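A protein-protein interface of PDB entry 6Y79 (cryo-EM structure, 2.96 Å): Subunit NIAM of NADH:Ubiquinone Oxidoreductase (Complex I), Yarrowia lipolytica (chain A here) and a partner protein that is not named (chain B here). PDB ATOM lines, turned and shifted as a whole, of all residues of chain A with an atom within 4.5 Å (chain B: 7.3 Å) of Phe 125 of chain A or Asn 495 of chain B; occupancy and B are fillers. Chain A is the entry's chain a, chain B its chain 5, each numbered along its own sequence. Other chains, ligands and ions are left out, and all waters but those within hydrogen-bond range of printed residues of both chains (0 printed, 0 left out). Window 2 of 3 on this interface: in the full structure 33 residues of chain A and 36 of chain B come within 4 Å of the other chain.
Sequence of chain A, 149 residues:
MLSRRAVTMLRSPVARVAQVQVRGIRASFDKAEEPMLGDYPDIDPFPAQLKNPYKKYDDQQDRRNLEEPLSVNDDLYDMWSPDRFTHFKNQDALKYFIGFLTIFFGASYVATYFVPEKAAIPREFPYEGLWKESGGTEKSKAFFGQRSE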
ATOM      1  N   ARG A 123     -27.844 -20.394 -17.265  1.00  0.00           N
ATOM      2  CA  ARG A 123     -27.297 -19.049 -17.358  1.00  0.00           C
ATOM      3  C   ARG A 123     -26.268 -18.926 -18.471  1.00  0.00           C
ATOM      4  O   ARG A 123     -25.599 -19.890 -18.850  1.00  0.00           O
ATOM      5  CB  ARG A 123     -26.675 -18.625 -16.030  1.00  0.00           C
ATOM      6  CG  ARG A 123     -25.556 -19.501 -15.557  1.00  0.00           C
ATOM      7  CD  ARG A 123     -25.021 -19.033 -14.219  1.00  0.00           C
ATOM      8  NE  ARG A 123     -23.803 -19.751 -13.877  1.00  0.00           N
ATOM      9  CZ  ARG A 123     -22.582 -19.315 -14.165  1.00  0.00           C
ATOM     10  NH1 ARG A 123     -21.523 -20.033 -13.833  1.00  0.00           N
ATOM     11  NH2 ARG A 123     -22.422 -18.157 -14.783  1.00  0.00           N
ATOM     12  N   GLU A 124     -26.163 -17.712 -18.996  1.00  0.00           N
ATOM     13  CA  GLU A 124     -25.427 -17.400 -20.204  1.00  0.00           C
ATOM     14  C   GLU A 124     -24.281 -16.444 -19.879  1.00  0.00           C
ATOM     15  O   GLU A 124     -24.135 -15.962 -18.755  1.00  0.00           O
ATOM     16  CB  GLU A 124     -26.365 -16.823 -21.270  1.00  0.00           C
ATOM     17  CG  GLU A 124     -27.221 -15.613 -20.858  1.00  0.00           C
ATOM     18  CD  GLU A 124     -28.507 -15.967 -20.115  1.00  0.00           C
ATOM     19  OE1 GLU A 124     -29.261 -15.034 -19.761  1.00  0.00           O
ATOM     20  OE2 GLU A 124     -28.759 -17.166 -19.888  1.00  0.00           O
ATOM     21  N   PHE A 125     -23.460 -16.156 -20.889  1.00  0.00           N
ATOM     22  CA  PHE A 125     -22.111 -15.673 -20.668  1.00  0.00           C
ATOM     23  C   PHE A 125     -21.756 -14.536 -21.615  1.00  0.00           C
ATOM     24  O   PHE A 125     -22.219 -14.521 -22.763  1.00  0.00           O
ATOM     25  CB  PHE A 125     -21.125 -16.834 -20.850  1.00  0.00           C
ATOM     26  CG  PHE A 125     -21.292 -17.926 -19.840  1.00  0.00           C
ATOM     27  CD1 PHE A 125     -20.664 -17.848 -18.612  1.00  0.00           C
ATOM     28  CD2 PHE A 125     -22.100 -19.023 -20.109  1.00  0.00           C
ATOM     29  CE1 PHE A 125     -20.829 -18.843 -17.676  1.00  0.00           C
ATOM     30  CE2 PHE A 125     -22.271 -20.020 -19.175  1.00  0.00           C
ATOM     31  CZ  PHE A 125     -21.638 -19.926 -17.959  1.00  0.00           C
ATOM     32  N   PRO A 126     -20.949 -13.579 -21.177  1.00  0.00           N
ATOM     33  CA  PRO A 126     -20.562 -12.470 -22.048  1.00  0.00           C
ATOM     34  C   PRO A 126     -19.404 -12.866 -22.957  1.00  0.00           C
ATOM     35  O   PRO A 126     -18.914 -13.999 -22.928  1.00  0.00           O
ATOM     36  CB  PRO A 126     -20.149 -11.389 -21.053  1.00  0.00           C
ATOM     37  CG  PRO A 126     -19.563 -12.158 -19.936  1.00  0.00           C
ATOM     38  CD  PRO A 126     -20.392 -13.409 -19.822  1.00  0.00           C
ATOM     39  N   TYR A 127     -18.976 -11.885 -23.764  1.00  0.00           N
ATOM     40  CA  TYR A 127     -17.898 -12.019 -24.751  1.00  0.00           C
ATOM     41  C   TYR A 127     -18.152 -13.172 -25.710  1.00  0.00           C
ATOM     42  O   TYR A 127     -17.227 -13.910 -26.072  1.00  0.00           O
ATOM     43  CB  TYR A 127     -16.541 -12.150 -24.072  1.00  0.00           C
ATOM     44  CG  TYR A 127     -16.206 -10.892 -23.338  1.00  0.00           C
ATOM     45  CD1 TYR A 127     -15.735  -9.785 -24.023  1.00  0.00           C
ATOM     46  CD2 TYR A 127     -16.422 -10.786 -21.972  1.00  0.00           C
ATOM     47  CE1 TYR A 127     -15.459  -8.621 -23.373  1.00  0.00           C
ATOM     48  CE2 TYR A 127     -16.146  -9.625 -21.308  1.00  0.00           C
ATOM     49  CZ  TYR A 127     -15.663  -8.548 -22.015  1.00  0.00           C
ATOM     50  OH  TYR A 127     -15.389  -7.386 -21.367  1.00  0.00           O
ATOM     51  N   GLY A 129     -19.978 -15.857 -25.036  1.00  0.00           N
ATOM     52  CA  GLY A 129     -19.794 -17.098 -24.313  1.00  0.00           C
ATOM     53  C   GLY A 129     -18.350 -17.458 -24.049  1.00  0.00           C
ATOM     54  O   GLY A 129     -17.993 -18.633 -24.164  1.00  0.00           O
ATOM     55  N   LEU A 130     -17.500 -16.458 -23.779  1.00  0.00           N
ATOM     56  CA  LEU A 130     -16.128 -16.642 -23.273  1.00  0.00           C
ATOM     57  C   LEU A 130     -15.260 -17.519 -24.170  1.00  0.00           C
ATOM     58  O   LEU A 130     -14.374 -18.219 -23.672  1.00  0.00           O
ATOM     59  CB  LEU A 130     -16.131 -17.234 -21.864  1.00  0.00           C
ATOM     60  CG  LEU A 130     -16.209 -16.330 -20.645  1.00  0.00           C
ATOM     61  CD1 LEU A 130     -17.604 -15.802 -20.460  1.00  0.00           C
ATOM     62  CD2 LEU A 130     -15.776 -17.110 -19.428  1.00  0.00           C
ATOM     63  N   GLN A 146     -19.772 -21.273 -25.140  1.00  0.00           N
ATOM     64  CA  GLN A 146     -20.780 -21.287 -24.087  1.00  0.00           C
ATOM     65  C   GLN A 146     -22.092 -20.705 -24.604  1.00  0.00           C
ATOM     66  O   GLN A 146     -22.270 -20.559 -25.817  1.00  0.00           O
ATOM     67  CB  GLN A 146     -20.290 -20.523 -22.856  1.00  0.00           C
ATOM     68  CG  GLN A 146     -18.969 -21.033 -22.278  1.00  0.00           C
ATOM     69  CD  GLN A 146     -19.100 -22.379 -21.633  1.00  0.00           C
ATOM     70  OE1 GLN A 146     -20.030 -22.610 -20.882  1.00  0.00           O
ATOM     71  NE2 GLN A 146     -18.169 -23.280 -21.920  1.00  0.00           N
ATOM     72  N   ARG A 147     -23.015 -20.381 -23.692  1.00  0.00           N
ATOM     73  CA  ARG A 147     -24.407 -20.134 -24.070  1.00  0.00           C
ATOM     74  C   ARG A 147     -24.611 -18.806 -24.791  1.00  0.00           C
ATOM     75  O   ARG A 147     -25.511 -18.711 -25.636  1.00  0.00           O
ATOM     76  CB  ARG A 147     -25.305 -20.171 -22.835  1.00  0.00           C
ATOM     77  CG  ARG A 147     -25.892 -21.531 -22.521  1.00  0.00           C
ATOM     78  CD  ARG A 147     -24.879 -22.339 -21.768  1.00  0.00           C
ATOM     79  NE  ARG A 147     -25.398 -23.560 -21.163  1.00  0.00           N
ATOM     80  CZ  ARG A 147     -25.712 -23.686 -19.879  1.00  0.00           C
ATOM     81  NH1 ARG A 147     -25.575 -22.659 -19.053  1.00  0.00           N
ATOM     82  NH2 ARG A 147     -26.156 -24.845 -19.420  1.00  0.00           N
ATOM     83  N   SER A 148     -23.805 -17.791 -24.468  1.00  0.00           N
ATOM     84  CA  SER A 148     -23.990 -16.388 -24.881  1.00  0.00           C
ATOM     85  C   SER A 148     -25.383 -15.861 -24.540  1.00  0.00           C
ATOM     86  O   SER A 148     -25.548 -14.693 -24.186  1.00  0.00           O
ATOM     87  CB  SER A 148     -23.721 -16.202 -26.380  1.00  0.00           C
ATOM     88  OG  SER A 148     -22.478 -16.761 -26.748  1.00  0.00           O
ATOM     89  N   GLU B 271     -13.617 -33.015 -16.463  1.00  0.00           N
ATOM     90  CA  GLU B 271     -14.657 -32.068 -16.891  1.00  0.00           C
ATOM     91  C   GLU B 271     -14.995 -32.239 -18.351  1.00  0.00           C
ATOM     92  O   GLU B 271     -16.149 -32.090 -18.747  1.00  0.00           O
ATOM     93  CB  GLU B 271     -14.207 -30.617 -16.683  1.00  0.00           C
ATOM     94  CG  GLU B 271     -14.111 -30.165 -15.277  1.00  0.00           C
ATOM     95  CD  GLU B 271     -15.457 -30.109 -14.599  1.00  0.00           C
ATOM     96  OE1 GLU B 271     -16.472 -29.781 -15.240  1.00  0.00           O
ATOM     97  OE2 GLU B 271     -15.480 -30.422 -13.404  1.00  0.00           O
ATOM     98  N   SER B 323     -20.416 -32.344 -10.860  1.00  0.00           N
ATOM     99  CA  SER B 323     -19.369 -31.374 -11.205  1.00  0.00           C
ATOM    100  C   SER B 323     -19.244 -30.280 -10.149  1.00  0.00           C
ATOM    101  O   SER B 323     -19.281 -29.085 -10.445  1.00  0.00           O
ATOM    102  CB  SER B 323     -19.597 -30.765 -12.582  1.00  0.00           C
ATOM    103  OG  SER B 323     -19.632 -31.758 -13.579  1.00  0.00           O
ATOM    104  N   TYR B 407     -28.280 -28.561 -13.516  1.00  0.00           N
ATOM    105  CA  TYR B 407     -28.859 -28.168 -14.794  1.00  0.00           C
ATOM    106  C   TYR B 407     -29.549 -29.338 -15.476  1.00  0.00           C
ATOM    107  O   TYR B 407     -30.588 -29.155 -16.113  1.00  0.00           O
ATOM    108  CB  TYR B 407     -27.789 -27.598 -15.711  1.00  0.00           C
ATOM    109  CG  TYR B 407     -27.280 -26.248 -15.301  1.00  0.00           C
ATOM    110  CD1 TYR B 407     -28.100 -25.129 -15.344  1.00  0.00           C
ATOM    111  CD2 TYR B 407     -25.975 -26.087 -14.891  1.00  0.00           C
ATOM    112  CE1 TYR B 407     -27.625 -23.884 -14.972  1.00  0.00           C
ATOM    113  CE2 TYR B 407     -25.493 -24.858 -14.528  1.00  0.00           C
ATOM    114  CZ  TYR B 407     -26.316 -23.760 -14.563  1.00  0.00           C
ATOM    115  OH  TYR B 407     -25.814 -22.537 -14.188  1.00  0.00           O
ATOM    116  N   SER B 408     -28.963 -30.528 -15.392  1.00  0.00           N
ATOM    117  CA  SER B 408     -29.521 -31.709 -16.038  1.00  0.00           C
ATOM    118  C   SER B 408     -30.799 -32.157 -15.347  1.00  0.00           C
ATOM    119  O   SER B 408     -31.040 -31.850 -14.181  1.00  0.00           O
ATOM    120  CB  SER B 408     -28.510 -32.843 -16.049  1.00  0.00           C
ATOM    121  OG  SER B 408     -29.115 -34.070 -16.394  1.00  0.00           O
ATOM    122  N   ILE B 492     -13.728 -25.638 -13.126  1.00  0.00           N
ATOM    123  CA  ILE B 492     -15.004 -26.141 -13.610  1.00  0.00           C
ATOM    124  C   ILE B 492     -15.278 -25.526 -14.974  1.00  0.00           C
ATOM    125  O   ILE B 492     -14.951 -24.355 -15.220  1.00  0.00           O
ATOM    126  CB  ILE B 492     -16.120 -25.810 -12.602  1.00  0.00           C
ATOM    127  CG1 ILE B 492     -15.754 -26.335 -11.220  1.00  0.00           C
ATOM    128  CG2 ILE B 492     -17.431 -26.482 -12.983  1.00  0.00           C
ATOM    129  CD1 ILE B 492     -15.673 -27.845 -11.154  1.00  0.00           C
ATOM    130  N   LEU B 493     -15.819 -26.334 -15.892  1.00  0.00           N
ATOM    131  CA  LEU B 493     -16.356 -25.798 -17.128  1.00  0.00           C
ATOM    132  C   LEU B 493     -17.536 -24.889 -16.791  1.00  0.00           C
ATOM    133  O   LEU B 493     -18.282 -25.174 -15.852  1.00  0.00           O
ATOM    134  CB  LEU B 493     -16.807 -26.926 -18.045  1.00  0.00           C
ATOM    135  CG  LEU B 493     -15.772 -27.720 -18.826  1.00  0.00           C
ATOM    136  CD1 LEU B 493     -16.503 -28.762 -19.634  1.00  0.00           C
ATOM    137  CD2 LEU B 493     -14.994 -26.805 -19.730  1.00  0.00           C
ATOM    138  N   PRO B 494     -17.734 -23.795 -17.537  1.00  0.00           N
ATOM    139  CA  PRO B 494     -18.736 -22.796 -17.124  1.00  0.00           C
ATOM    140  C   PRO B 494     -20.182 -23.280 -17.144  1.00  0.00           C
ATOM    141  O   PRO B 494     -21.019 -22.652 -16.489  1.00  0.00           O
ATOM    142  CB  PRO B 494     -18.515 -21.653 -18.119  1.00  0.00           C
ATOM    143  CG  PRO B 494     -17.114 -21.804 -18.553  1.00  0.00           C
ATOM    144  CD  PRO B 494     -16.891 -23.283 -18.628  1.00  0.00           C
ATOM    145  N   ASN B 495     -20.497 -24.383 -17.820  1.00  0.00           N
ATOM    146  CA  ASN B 495     -21.847 -24.927 -17.796  1.00  0.00           C
ATOM    147  C   ASN B 495     -22.041 -26.028 -16.777  1.00  0.00           C
ATOM    148  O   ASN B 495     -23.175 -26.268 -16.352  1.00  0.00           O
ATOM    149  CB  ASN B 495     -22.222 -25.473 -19.165  1.00  0.00           C
ATOM    150  CG  ASN B 495     -22.391 -24.391 -20.149  1.00  0.00           C
ATOM    151  OD1 ASN B 495     -22.570 -23.241 -19.756  1.00  0.00           O
ATOM    152  ND2 ASN B 495     -22.314 -24.716 -21.432  1.00  0.00           N
ATOM    153  N   ASN B 496     -20.974 -26.712 -16.395  1.00  0.00           N
ATOM    154  CA  ASN B 496     -21.079 -27.712 -15.355  1.00  0.00           C
ATOM    155  C   ASN B 496     -21.118 -27.096 -13.962  1.00  0.00           C
ATOM    156  O   ASN B 496     -21.395 -27.808 -12.990  1.00  0.00           O
ATOM    157  CB  ASN B 496     -19.924 -28.693 -15.525  1.00  0.00           C
ATOM    158  CG  ASN B 496     -20.029 -29.487 -16.814  1.00  0.00           C
ATOM    159  OD1 ASN B 496     -20.567 -30.599 -16.824  1.00  0.00           O
ATOM    160  ND2 ASN B 496     -19.535 -28.918 -17.915  1.00  0.00           N
ATOM    161  N   PHE B 497     -20.884 -25.789 -13.854  1.00  0.00           N
ATOM    162  CA  PHE B 497     -20.945 -25.062 -12.593  1.00  0.00           C
ATOM    163  C   PHE B 497     -22.382 -24.643 -12.318  1.00  0.00           C
ATOM    164  O   PHE B 497     -22.937 -23.812 -13.040  1.00  0.00           O
ATOM    165  CB  PHE B 497     -20.039 -23.842 -12.660  1.00  0.00           C
ATOM    166  CG  PHE B 497     -19.973 -23.075 -11.388  1.00  0.00           C
ATOM    167  CD1 PHE B 497     -19.253 -23.563 -10.315  1.00  0.00           C
ATOM    168  CD2 PHE B 497     -20.625 -21.865 -11.262  1.00  0.00           C
ATOM    169  CE1 PHE B 497     -19.183 -22.861  -9.140  1.00  0.00           C
ATOM    170  CE2 PHE B 497     -20.560 -21.157 -10.090  1.00  0.00           C
ATOM    171  CZ  PHE B 497     -19.837 -21.655  -9.028  1.00  0.00           C
ATOM    172  N   SER B 498     -22.972 -25.174 -11.247  1.00  0.00           N
ATOM    173  CA  SER B 498     -24.382 -24.956 -10.951  1.00  0.00           C
ATOM    174  C   SER B 498     -24.610 -24.451  -9.531  1.00  0.00           C
ATOM    175  O   SER B 498     -25.682 -24.655  -8.970  1.00  0.00           O
ATOM    176  CB  SER B 498     -25.181 -26.237 -11.180  1.00  0.00           C
ATOM    177  OG  SER B 498     -26.554 -26.028 -10.908  1.00  0.00           O
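The backbone carbonyl oxygen (O) of Arg 123 of chain A is in hydrogen-bond range of the guanidinium group (NH1) of Arg 147 of chain A, 2.8 Å away. OH of Tyr 407 of chain B lies close to O of Phe 497 of chain B, 3.3 Å away. N of Gln 146 of chain A sits close to O of Gly 129 of chain A (3.3 Å).
The side-chain amide oxygen of Gln 146 of chain A sits close to the side-chain amide oxygen of Asn 495 of chain B (2.8 Å). NH1 of Arg 147 of chain A is in hydrogen-bond range of OD1 of Asn 495 of chain B (3.1 Å). The guanidinium group of Arg 123 of chain A lies close to the side-chain hydroxyl of Tyr 407 of chain B (3.5 Å).
Hydrophobic or aromatic side chains of chain B that line the printed part of chain A: Tyr 407, Pro 494 and Phe 497. Among the printed residues, 8 pairs touch across the chains. Among the printed residues, no Asp or Glu carboxylate lies within 4 Å of a Lys or Arg side-chain nitrogen of the other chain.
Printed residues of chain B within 4 Å of Arg 123 of chain A: Tyr 407 (3.3 Å), Pro 494 (3.8 Å) and Phe 497 (3.3 Å). Phe 125 of chain A touches just these residues of chain B: Pro 494 and Asn 495. Of the printed residues of chain B, Gln 146 of chain A touches Pro 494 and Asn 495. Printed residues of chain B within 4 Å of Arg 147 of chain A: Asn 495. Printed residues of chain A within 4 Å of Tyr 407 of chain B: Arg 123 (3.3 Å). Leu 493 of chain B touches none of the printed residues of chain A. Asn 495 of chain B touches just these residues of chain A: Phe 125, Gln 146 and Arg 147. The nearest residue of chain B that does not touch Phe 125 of chain A is Tyr 407 of chain B (6.2 Å). The nearest printed residue of chain A that does not touch Tyr 407 of chain B is Arg 147 of chain A (4.5 Å).
NH1 of Arg 123 of chain A touches O of Pro 494 of chain B, 3.8 Å away. Arg 123 of chain A touches Phe 497 of chain B (NH1 to CD2, 3.3 Å). CZ of Phe 125 of chain A touches O of Pro 494 of chain B (3.2 Å). CE2 of Phe 125 of chain A touches OD1 of Asn 495 of chain B, 3.3 Å away. Pro 494 of chain B touches Gln 146 of chain A.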
